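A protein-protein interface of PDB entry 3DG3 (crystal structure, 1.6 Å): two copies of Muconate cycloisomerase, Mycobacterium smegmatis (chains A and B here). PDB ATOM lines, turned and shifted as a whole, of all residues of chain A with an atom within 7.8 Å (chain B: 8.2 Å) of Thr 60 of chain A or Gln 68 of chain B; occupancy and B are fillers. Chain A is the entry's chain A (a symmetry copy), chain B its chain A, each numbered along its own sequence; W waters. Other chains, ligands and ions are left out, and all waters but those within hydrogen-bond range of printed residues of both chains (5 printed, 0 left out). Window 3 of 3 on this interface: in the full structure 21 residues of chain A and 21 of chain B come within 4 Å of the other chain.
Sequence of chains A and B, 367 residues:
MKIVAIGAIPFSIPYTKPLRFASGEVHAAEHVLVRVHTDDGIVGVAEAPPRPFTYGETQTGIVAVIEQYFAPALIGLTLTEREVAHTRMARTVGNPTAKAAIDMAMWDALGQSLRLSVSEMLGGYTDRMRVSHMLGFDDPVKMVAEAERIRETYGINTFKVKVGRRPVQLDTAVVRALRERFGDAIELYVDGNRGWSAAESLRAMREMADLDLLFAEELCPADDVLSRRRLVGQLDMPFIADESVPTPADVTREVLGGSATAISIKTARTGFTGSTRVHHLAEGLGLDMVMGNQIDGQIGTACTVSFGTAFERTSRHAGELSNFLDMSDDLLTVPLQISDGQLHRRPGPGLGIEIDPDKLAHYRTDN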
ATOM      1  N   PRO A  10     -24.303  24.228 -22.014  1.00  0.00           N
ATOM      2  CA  PRO A  10     -24.802  24.359 -20.645  1.00  0.00           C
ATOM      3  C   PRO A  10     -26.295  24.662 -20.657  1.00  0.00           C
ATOM      4  O   PRO A  10     -26.775  25.404 -21.517  1.00  0.00           O
ATOM      5  CB  PRO A  10     -23.986  25.525 -20.098  1.00  0.00           C
ATOM      6  CG  PRO A  10     -23.844  26.403 -21.306  1.00  0.00           C
ATOM      7  CD  PRO A  10     -23.496  25.403 -22.393  1.00  0.00           C
ATOM      8  N   GLU A  30     -28.152  22.362 -13.190  1.00  0.00           N
ATOM      9  CA  GLU A  30     -27.307  23.117 -14.105  1.00  0.00           C
ATOM     10  C   GLU A  30     -26.324  22.124 -14.704  1.00  0.00           C
ATOM     11  O   GLU A  30     -25.192  21.995 -14.239  1.00  0.00           O
ATOM     12  CB  GLU A  30     -26.559  24.218 -13.349  1.00  0.00           C
ATOM     13  CG  GLU A  30     -27.464  25.069 -12.470  1.00  0.00           C
ATOM     14  CD  GLU A  30     -26.721  26.195 -11.777  1.00  0.00           C
ATOM     15  OE1 GLU A  30     -25.627  25.941 -11.230  1.00  0.00           O
ATOM     16  OE2 GLU A  30     -27.238  27.333 -11.770  1.00  0.00           O
ATOM     17  N   VAL A  32     -24.647  19.947 -18.353  1.00  0.00           N
ATOM     18  CA  VAL A  32     -24.049  20.221 -19.649  1.00  0.00           C
ATOM     19  C   VAL A  32     -24.443  19.121 -20.620  1.00  0.00           C
ATOM     20  O   VAL A  32     -24.228  17.939 -20.354  1.00  0.00           O
ATOM     21  CB  VAL A  32     -22.506  20.265 -19.558  1.00  0.00           C
ATOM     22  CG1 VAL A  32     -21.911  20.482 -20.942  1.00  0.00           C
ATOM     23  CG2 VAL A  32     -22.072  21.375 -18.610  1.00  0.00           C
ATOM     24  N   PRO A  50     -22.313  18.904 -13.187  1.00  0.00           N
ATOM     25  CA  PRO A  50     -21.205  19.466 -12.408  1.00  0.00           C
ATOM     26  C   PRO A  50     -21.483  19.364 -10.913  1.00  0.00           C
ATOM     27  O   PRO A  50     -22.486  19.881 -10.417  1.00  0.00           O
ATOM     28  CB  PRO A  50     -21.132  20.908 -12.900  1.00  0.00           C
ATOM     29  CG  PRO A  50     -22.557  21.223 -13.212  1.00  0.00           C
ATOM     30  CD  PRO A  50     -23.053  19.963 -13.898  1.00  0.00           C
ATOM     31  N   GLU A  57     -15.813  19.682 -10.282  1.00  0.00           N
ATOM     32  CA  GLU A  57     -16.112  20.230 -11.600  1.00  0.00           C
ATOM     33  C   GLU A  57     -17.188  21.307 -11.495  1.00  0.00           C
ATOM     34  O   GLU A  57     -18.035  21.266 -10.600  1.00  0.00           O
ATOM     35  CB  GLU A  57     -16.613  19.127 -12.542  1.00  0.00           C
ATOM     36  CG  GLU A  57     -15.586  18.071 -12.906  1.00  0.00           C
ATOM     37  CD  GLU A  57     -16.161  16.998 -13.816  1.00  0.00           C
ATOM     38  OE1 GLU A  57     -16.959  16.168 -13.332  1.00  0.00           O
ATOM     39  OE2 GLU A  57     -15.821  16.989 -15.016  1.00  0.00           O
ATOM     40  N   THR A  58     -17.139  22.279 -12.401  1.00  0.00           N
ATOM     41  CA  THR A  58     -18.138  23.341 -12.439  1.00  0.00           C
ATOM     42  C   THR A  58     -18.740  23.297 -13.834  1.00  0.00           C
ATOM     43  O   THR A  58     -18.153  22.722 -14.751  1.00  0.00           O
ATOM     44  CB  THR A  58     -17.519  24.744 -12.221  1.00  0.00           C
ATOM     45  OG1 THR A  58     -16.644  25.060 -13.312  1.00  0.00           O
ATOM     46  CG2 THR A  58     -16.747  24.786 -10.911  1.00  0.00           C
ATOM     47  N   GLN A  59     -19.911  23.897 -14.004  1.00  0.00           N
ATOM     48  CA  GLN A  59     -20.542  23.900 -15.314  1.00  0.00           C
ATOM     49  C   GLN A  59     -19.615  24.585 -16.320  1.00  0.00           C
ATOM     50  O   GLN A  59     -19.415  24.096 -17.431  1.00  0.00           O
ATOM     51  CB  GLN A  59     -21.888  24.623 -15.247  1.00  0.00           C
ATOM     52  CG  GLN A  59     -22.714  24.510 -16.512  1.00  0.00           C
ATOM     53  CD  GLN A  59     -24.043  25.228 -16.390  1.00  0.00           C
ATOM     54  OE1 GLN A  59     -24.092  26.395 -16.002  1.00  0.00           O
ATOM     55  NE2 GLN A  59     -25.129  24.536 -16.720  1.00  0.00           N
ATOM     56  N   THR A  60     -19.037  25.712 -15.919  1.00  0.00           N
ATOM     57  CA  THR A  60     -18.125  26.444 -16.789  1.00  0.00           C
ATOM     58  C   THR A  60     -16.883  25.606 -17.091  1.00  0.00           C
ATOM     59  O   THR A  60     -16.398  25.579 -18.223  1.00  0.00           O
ATOM     60  CB  THR A  60     -17.674  27.769 -16.140  1.00  0.00           C
ATOM     61  OG1 THR A  60     -18.813  28.612 -15.926  1.00  0.00           O
ATOM     62  CG2 THR A  60     -16.670  28.484 -17.036  1.00  0.00           C
ATOM     63  N   GLY A  61     -16.377  24.918 -16.068  1.00  0.00           N
ATOM     64  CA  GLY A  61     -15.190  24.093 -16.228  1.00  0.00           C
ATOM     65  C   GLY A  61     -15.358  22.907 -17.159  1.00  0.00           C
ATOM     66  O   GLY A  61     -14.439  22.560 -17.902  1.00  0.00           O
ATOM     67  N   ILE A  62     -16.530  22.277 -17.115  1.00  0.00           N
ATOM     68  CA  ILE A  62     -16.820  21.127 -17.966  1.00  0.00           C
ATOM     69  C   ILE A  62     -16.814  21.550 -19.434  1.00  0.00           C
ATOM     70  O   ILE A  62     -16.199  20.905 -20.282  1.00  0.00           O
ATOM     71  CB  ILE A  62     -18.201  20.512 -17.611  1.00  0.00           C
ATOM     72  CG1 ILE A  62     -18.128  19.820 -16.243  1.00  0.00           C
ATOM     73  CG2 ILE A  62     -18.627  19.514 -18.685  1.00  0.00           C
ATOM     74  CD1 ILE A  62     -19.481  19.369 -15.705  1.00  0.00           C
ATOM     75  N   VAL A  63     -17.511  22.639 -19.734  1.00  0.00           N
ATOM     76  CA  VAL A  63     -17.564  23.130 -21.101  1.00  0.00           C
ATOM     77  C   VAL A  63     -16.155  23.477 -21.573  1.00  0.00           C
ATOM     78  O   VAL A  63     -15.776  23.181 -22.704  1.00  0.00           O
ATOM     79  CB  VAL A  63     -18.459  24.386 -21.202  1.00  0.00           C
ATOM     80  CG1 VAL A  63     -18.386  24.971 -22.607  1.00  0.00           C
ATOM     81  CG2 VAL A  63     -19.895  24.022 -20.854  1.00  0.00           C
ATOM     82  N   ALA A  64     -15.375  24.090 -20.689  1.00  0.00           N
ATOM     83  CA  ALA A  64     -14.014  24.485 -21.027  1.00  0.00           C
ATOM     84  C   ALA A  64     -13.095  23.307 -21.334  1.00  0.00           C
ATOM     85  O   ALA A  64     -12.392  23.311 -22.344  1.00  0.00           O
ATOM     86  CB  ALA A  64     -13.423  25.326 -19.903  1.00  0.00           C
ATOM     87  N   VAL A  65     -13.098  22.290 -20.477  1.00  0.00           N
ATOM     88  CA  VAL A  65     -12.217  21.155 -20.711  1.00  0.00           C
ATOM     89  C   VAL A  65     -12.611  20.378 -21.966  1.00  0.00           C
ATOM     90  O   VAL A  65     -11.754  19.850 -22.669  1.00  0.00           O
ATOM     91  CB  VAL A  65     -12.168  20.210 -19.476  1.00  0.00           C
ATOM     92  CG1 VAL A  65     -13.438  19.372 -19.388  1.00  0.00           C
ATOM     93  CG2 VAL A  65     -10.928  19.330 -19.552  1.00  0.00           C
ATOM     94  N   ILE A  66     -13.906  20.323 -22.262  1.00  0.00           N
ATOM     95  CA  ILE A  66     -14.359  19.613 -23.451  1.00  0.00           C
ATOM     96  C   ILE A  66     -13.997  20.379 -24.724  1.00  0.00           C
ATOM     97  O   ILE A  66     -13.445  19.807 -25.664  1.00  0.00           O
ATOM     98  CB  ILE A  66     -15.888  19.376 -23.416  1.00  0.00           C
ATOM     99  CG1 ILE A  66     -16.221  18.370 -22.310  1.00  0.00           C
ATOM    100  CG2 ILE A  66     -16.372  18.844 -24.766  1.00  0.00           C
ATOM    101  CD1 ILE A  66     -17.695  18.051 -22.176  1.00  0.00           C
ATOM    102  N   GLU A  67     -14.294  21.674 -24.745  1.00  0.00           N
ATOM    103  CA  GLU A  67     -14.000  22.489 -25.922  1.00  0.00           C
ATOM    104  C   GLU A  67     -12.507  22.692 -26.152  1.00  0.00           C
ATOM    105  O   GLU A  67     -12.037  22.672 -27.289  1.00  0.00           O
ATOM    106  CB  GLU A  67     -14.674  23.865 -25.810  1.00  0.00           C
ATOM    107  CG  GLU A  67     -16.187  23.828 -25.641  1.00  0.00           C
ATOM    108  CD  GLU A  67     -16.823  25.205 -25.750  1.00  0.00           C
ATOM    109  OE1 GLU A  67     -16.179  26.196 -25.347  1.00  0.00           O
ATOM    110  OE2 GLU A  67     -17.973  25.294 -26.231  1.00  0.00           O
ATOM    111  N   GLN A  68     -11.759  22.871 -25.067  1.00  0.00           N
ATOM    112  CA  GLN A  68     -10.326  23.125 -25.159  1.00  0.00           C
ATOM    113  C   GLN A  68      -9.394  21.923 -25.194  1.00  0.00           C
ATOM    114  O   GLN A  68      -8.307  22.002 -25.766  1.00  0.00           O
ATOM    115  CB  GLN A  68      -9.900  24.032 -24.007  1.00  0.00           C
ATOM    116  CG  GLN A  68     -10.510  25.418 -24.043  1.00  0.00           C
ATOM    117  CD  GLN A  68     -10.238  26.186 -22.769  1.00  0.00           C
ATOM    118  OE1 GLN A  68      -9.197  26.006 -22.140  1.00  0.00           O
ATOM    119  NE2 GLN A  68     -11.168  27.052 -22.386  1.00  0.00           N
ATOM    120  N   ILE B   6     -11.595  39.050  -3.929  1.00  0.00           N
ATOM    121  CA  ILE B   6     -10.622  38.066  -4.388  1.00  0.00           C
ATOM    122  C   ILE B   6     -10.754  37.986  -5.902  1.00  0.00           C
ATOM    123  O   ILE B   6     -11.832  37.694  -6.425  1.00  0.00           O
ATOM    124  CB  ILE B   6     -10.891  36.667  -3.780  1.00  0.00           C
ATOM    125  CG1 ILE B   6     -10.782  36.733  -2.255  1.00  0.00           C
ATOM    126  CG2 ILE B   6      -9.902  35.658  -4.349  1.00  0.00           C
ATOM    127  CD1 ILE B   6     -10.992  35.398  -1.564  1.00  0.00           C
ATOM    128  N   ALA B   8      -9.097  36.789  -9.908  1.00  0.00           N
ATOM    129  CA  ALA B   8      -8.328  35.783 -10.633  1.00  0.00           C
ATOM    130  C   ALA B   8      -8.097  36.289 -12.053  1.00  0.00           C
ATOM    131  O   ALA B   8      -9.026  36.342 -12.862  1.00  0.00           O
ATOM    132  CB  ALA B   8      -9.087  34.456 -10.658  1.00  0.00           C
ATOM    133  N   THR B  58      -7.835  23.750 -15.502  1.00  0.00           N
ATOM    134  CA  THR B  58      -7.541  24.494 -16.722  1.00  0.00           C
ATOM    135  C   THR B  58      -7.493  25.957 -16.316  1.00  0.00           C
ATOM    136  O   THR B  58      -8.000  26.330 -15.257  1.00  0.00           O
ATOM    137  CB  THR B  58      -8.641  24.325 -17.799  1.00  0.00           C
ATOM    138  OG1 THR B  58      -9.866  24.906 -17.333  1.00  0.00           O
ATOM    139  CG2 THR B  58      -8.856  22.852 -18.113  1.00  0.00           C
ATOM    140  N   THR B  60      -9.094  28.409 -17.618  1.00  0.00           N
ATOM    141  CA  THR B  60     -10.475  28.876 -17.582  1.00  0.00           C
ATOM    142  C   THR B  60     -11.186  28.355 -16.334  1.00  0.00           C
ATOM    143  O   THR B  60     -11.944  29.081 -15.689  1.00  0.00           O
ATOM    144  CB  THR B  60     -11.258  28.403 -18.824  1.00  0.00           C
ATOM    145  OG1 THR B  60     -10.662  28.952 -20.007  1.00  0.00           O
ATOM    146  CG2 THR B  60     -12.713  28.845 -18.734  1.00  0.00           C
ATOM    147  N   GLY B  61     -10.931  27.091 -15.999  1.00  0.00           N
ATOM    148  CA  GLY B  61     -11.557  26.478 -14.837  1.00  0.00           C
ATOM    149  C   GLY B  61     -11.163  27.087 -13.505  1.00  0.00           C
ATOM    150  O   GLY B  61     -11.992  27.204 -12.602  1.00  0.00           O
ATOM    151  N   ILE B  62      -9.894  27.468 -13.376  1.00  0.00           N
ATOM    152  CA  ILE B  62      -9.393  28.075 -12.146  1.00  0.00           C
ATOM    153  C   ILE B  62     -10.086  29.415 -11.906  1.00  0.00           C
ATOM    154  O   ILE B  62     -10.561  29.700 -10.807  1.00  0.00           O
ATOM    155  CB  ILE B  62      -7.858  28.295 -12.227  1.00  0.00           C
ATOM    156  CG1 ILE B  62      -7.133  26.943 -12.172  1.00  0.00           C
ATOM    157  CG2 ILE B  62      -7.391  29.190 -11.081  1.00  0.00           C
ATOM    158  CD1 ILE B  62      -5.638  27.031 -12.457  1.00  0.00           C
ATOM    159  N   VAL B  63     -10.137  30.244 -12.941  1.00  0.00           N
ATOM    160  CA  VAL B  63     -10.782  31.541 -12.818  1.00  0.00           C
ATOM    161  C   VAL B  63     -12.251  31.348 -12.454  1.00  0.00           C
ATOM    162  O   VAL B  63     -12.794  32.063 -11.614  1.00  0.00           O
ATOM    163  CB  VAL B  63     -10.686  32.332 -14.142  1.00  0.00           C
ATOM    164  CG1 VAL B  63     -11.491  33.623 -14.043  1.00  0.00           C
ATOM    165  CG2 VAL B  63      -9.227  32.640 -14.451  1.00  0.00           C
ATOM    166  N   ALA B  64     -12.885  30.360 -13.076  1.00  0.00           N
ATOM    167  CA  ALA B  64     -14.293  30.087 -12.823  1.00  0.00           C
ATOM    168  C   ALA B  64     -14.581  29.648 -11.391  1.00  0.00           C
ATOM    169  O   ALA B  64     -15.491  30.173 -10.749  1.00  0.00           O
ATOM    170  CB  ALA B  64     -14.802  29.036 -13.801  1.00  0.00           C
ATOM    171  N   VAL B  65     -13.810  28.695 -10.877  1.00  0.00           N
ATOM    172  CA  VAL B  65     -14.064  28.222  -9.524  1.00  0.00           C
ATOM    173  C   VAL B  65     -13.789  29.305  -8.482  1.00  0.00           C
ATOM    174  O   VAL B  65     -14.468  29.377  -7.460  1.00  0.00           O
ATOM    175  CB  VAL B  65     -13.243  26.939  -9.207  1.00  0.00           C
ATOM    176  CG1 VAL B  65     -11.781  27.283  -8.952  1.00  0.00           C
ATOM    177  CG2 VAL B  65     -13.858  26.217  -8.016  1.00  0.00           C
ATOM    178  N   ILE B  66     -12.807  30.162  -8.744  1.00  0.00           N
ATOM    179  CA  ILE B  66     -12.494  31.232  -7.805  1.00  0.00           C
ATOM    180  C   ILE B  66     -13.576  32.312  -7.817  1.00  0.00           C
ATOM    181  O   ILE B  66     -14.065  32.721  -6.764  1.00  0.00           O
ATOM    182  CB  ILE B  66     -11.125  31.878  -8.125  1.00  0.00           C
ATOM    183  CG1 ILE B  66     -10.007  30.872  -7.831  1.00  0.00           C
ATOM    184  CG2 ILE B  66     -10.926  33.139  -7.282  1.00  0.00           C
ATOM    185  CD1 ILE B  66      -8.610  31.390  -8.103  1.00  0.00           C
ATOM    186  N   GLU B  67     -13.959  32.758  -9.009  1.00  0.00           N
ATOM    187  CA  GLU B  67     -14.977  33.800  -9.124  1.00  0.00           C
ATOM    188  C   GLU B  67     -16.366  33.329  -8.707  1.00  0.00           C
ATOM    189  O   GLU B  67     -17.116  34.068  -8.070  1.00  0.00           O
ATOM    190  CB  GLU B  67     -15.047  34.332 -10.563  1.00  0.00           C
ATOM    191  CG  GLU B  67     -13.742  34.901 -11.103  1.00  0.00           C
ATOM    192  CD  GLU B  67     -13.917  35.603 -12.440  1.00  0.00           C
ATOM    193  OE1 GLU B  67     -14.780  35.173 -13.235  1.00  0.00           O
ATOM    194  OE2 GLU B  67     -13.183  36.580 -12.702  1.00  0.00           O
ATOM    195  N   GLN B  68     -16.700  32.090  -9.054  1.00  0.00           N
ATOM    196  CA  GLN B  68     -18.018  31.542  -8.757  1.00  0.00           C
ATOM    197  C   GLN B  68     -18.215  30.860  -7.411  1.00  0.00           C
ATOM    198  O   GLN B  68     -19.328  30.845  -6.884  1.00  0.00           O
ATOM    199  CB  GLN B  68     -18.415  30.560  -9.857  1.00  0.00           C
ATOM    200  CG  GLN B  68     -18.592  31.189 -11.224  1.00  0.00           C
ATOM    201  CD  GLN B  68     -18.756  30.146 -12.306  1.00  0.00           C
ATOM    202  OE1 GLN B  68     -19.309  29.074 -12.064  1.00  0.00           O
ATOM    203  NE2 GLN B  68     -18.285  30.455 -13.508  1.00  0.00           N
ATOM    204  N   TYR B  69     -17.153  30.299  -6.848  1.00  0.00           N
ATOM    205  CA  TYR B  69     -17.289  29.592  -5.584  1.00  0.00           C
ATOM    206  C   TYR B  69     -16.455  30.095  -4.414  1.00  0.00           C
ATOM    207  O   TYR B  69     -16.997  30.451  -3.370  1.00  0.00           O
ATOM    208  CB  TYR B  69     -16.997  28.102  -5.805  1.00  0.00           C
ATOM    209  CG  TYR B  69     -18.042  27.397  -6.642  1.00  0.00           C
ATOM    210  CD1 TYR B  69     -19.135  26.772  -6.044  1.00  0.00           C
ATOM    211  CD2 TYR B  69     -17.951  27.378  -8.033  1.00  0.00           C
ATOM    212  CE1 TYR B  69     -20.112  26.143  -6.810  1.00  0.00           C
ATOM    213  CE2 TYR B  69     -18.927  26.752  -8.811  1.00  0.00           C
ATOM    214  CZ  TYR B  69     -20.003  26.138  -8.190  1.00  0.00           C
ATOM    215  OH  TYR B  69     -20.972  25.521  -8.950  1.00  0.00           O
ATOM    216  N   PHE B  70     -15.138  30.122  -4.577  1.00  0.00           N
ATOM    217  CA  PHE B  70     -14.272  30.539  -3.481  1.00  0.00           C
ATOM    218  C   PHE B  70     -14.371  31.999  -3.053  1.00  0.00           C
ATOM    219  O   PHE B  70     -14.491  32.285  -1.862  1.00  0.00           O
ATOM    220  CB  PHE B  70     -12.817  30.178  -3.799  1.00  0.00           C
ATOM    221  CG  PHE B  70     -12.590  28.702  -4.000  1.00  0.00           C
ATOM    222  CD1 PHE B  70     -13.233  27.769  -3.188  1.00  0.00           C
ATOM    223  CD2 PHE B  70     -11.725  28.246  -4.988  1.00  0.00           C
ATOM    224  CE1 PHE B  70     -13.016  26.401  -3.362  1.00  0.00           C
ATOM    225  CE2 PHE B  70     -11.499  26.881  -5.171  1.00  0.00           C
ATOM    226  CZ  PHE B  70     -12.146  25.957  -4.356  1.00  0.00           C
ATOM    227  N   ALA B  71     -14.327  32.924  -4.006  1.00  0.00           N
ATOM    228  CA  ALA B  71     -14.409  34.340  -3.666  1.00  0.00           C
ATOM    229  C   ALA B  71     -15.642  34.664  -2.816  1.00  0.00           C
ATOM    230  O   ALA B  71     -15.518  35.195  -1.714  1.00  0.00           O
ATOM    231  CB  ALA B  71     -14.399  35.188  -4.934  1.00  0.00           C
ATOM    232  N   PRO B  72     -16.850  34.343  -3.309  1.00  0.00           N
ATOM    233  CA  PRO B  72     -18.028  34.654  -2.493  1.00  0.00           C
ATOM    234  C   PRO B  72     -18.073  33.956  -1.133  1.00  0.00           C
ATOM    235  O   PRO B  72     -18.683  34.460  -0.189  1.00  0.00           O
ATOM    236  CB  PRO B  72     -19.197  34.259  -3.403  1.00  0.00           C
ATOM    237  CG  PRO B  72     -18.614  33.202  -4.286  1.00  0.00           C
ATOM    238  CD  PRO B  72     -17.243  33.747  -4.597  1.00  0.00           C
ATOM    239  N   ALA B  73     -17.415  32.807  -1.021  1.00  0.00           N
ATOM    240  CA  ALA B  73     -17.408  32.069   0.237  1.00  0.00           C
ATOM    241  C   ALA B  73     -16.399  32.610   1.245  1.00  0.00           C
ATOM    242  O   ALA B  73     -16.529  32.364   2.443  1.00  0.00           O
ATOM    243  CB  ALA B  73     -17.128  30.591  -0.030  1.00  0.00           C
ATOM    244  N   THR B  92     -15.295  22.129  -1.509  1.00  0.00           N
ATOM    245  CA  THR B  92     -15.138  21.879  -2.934  1.00  0.00           C
ATOM    246  C   THR B  92     -13.996  20.882  -3.090  1.00  0.00           C
ATOM    247  O   THR B  92     -12.924  21.058  -2.511  1.00  0.00           O
ATOM    248  CB  THR B  92     -14.799  23.175  -3.701  1.00  0.00           C
ATOM    249  OG1 THR B  92     -15.886  24.099  -3.575  1.00  0.00           O
ATOM    250  CG2 THR B  92     -14.569  22.884  -5.177  1.00  0.00           C
HETATM  251  O   HOH W   1     -20.149  27.156 -13.517  1.00  0.00           O
HETATM  252  O   HOH W   2     -11.928  23.194 -16.872  1.00  0.00           O
HETATM  253  O   HOH W   3      -8.080  27.216 -20.194  1.00  0.00           O
HETATM  254  O   HOH W   4     -21.041  25.171 -11.699  1.00  0.00           O
HETATM  255  O   HOH W   5     -13.997  25.272 -12.728  1.00  0.00           O
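Thr 60 of chain A touches Ala 64 of chain B, and with the chains exchanged Ala 64 of chain A touches Thr 60 of chain B.
Thr 60 of chain A touches Gln 68 of chain B, and with the chains exchanged Gln 68 of chain A touches Thr 60 of chain B.
Of the printed residues of chain B, Thr 58 of chain A touches Tyr 69.
Of the printed residues of chain A, Thr 60 of chain B touches Ala 64 (3.8 Å) and Gln 68 (3.1 Å).
Printed residues of chain A within 4 Å of Ala 64 of chain B: Thr 60.
Of chain A, only Thr 60 comes within 4 Å of Gln 68 of chain B.
Pro 72 of chain B touches none of the printed residues of chain A.
The backbone NH (N) of Gly 61 of chain A sits at hydrogen-bond distance from the side-chain hydroxyl (OG1) of Thr 58 of chain A (2.8 Å).
Water W1 lies within hydrogen-bond range of the side-chain amide oxygen (OE1) of Gln 68 of chain B, the backbone NH (N) of Thr 60 of chain A and the backbone NH (N) of Gln 59 of chain A.
Water W3 bridges the side-chain amide oxygen of Gln 68 of chain A (2.5 Å) and the backbone NH of Thr 60 of chain B (3.0 Å).
Water W2 lies within hydrogen-bond range of OG1 of Thr 58 of chain B (2.7 Å) and O of Gly 61 of chain A (2.8 Å).
Water W5 bridges OG1 of Thr 58 of chain A (2.7 Å) and O of Gly 61 of chain B (2.8 Å).
Water W4 bridges the side-chain hydroxyl (OH) of Tyr 69 of chain B (2.8 Å) and the backbone NH (N) of Gln 59 of chain A (2.9 Å).
NE2 of Gln 68 of chain A is in hydrogen-bond range of OG1 of Thr 60 of chain B.
NE2 of Gln 68 of chain B lies within hydrogen-bond range of OG1 of Thr 60 of chain A.
Of the 16 printed residues of chain A, 4 touch a printed residue of chain B.
Of the 18 printed residues of chain B, 4 touch a printed residue of chain A.
Hydrophobic or aromatic side chains of chain B that line the printed part of chain A: Ala 64 and Tyr 69.
Among the printed residues, no Asp or Glu carboxylate lies within 4 Å of a Lys or Arg side-chain nitrogen of the other chain.
CG2 of Thr 58 of chain A touches CE2 of Tyr 69 of chain B, 3.6 Å away.
CB of Ala 64 of chain B touches CG2 of Thr 60 of chain A, 3.8 Å away.
CB of Ala 64 of chain A touches CG2 of Thr 60 of chain B, 3.8 Å away.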
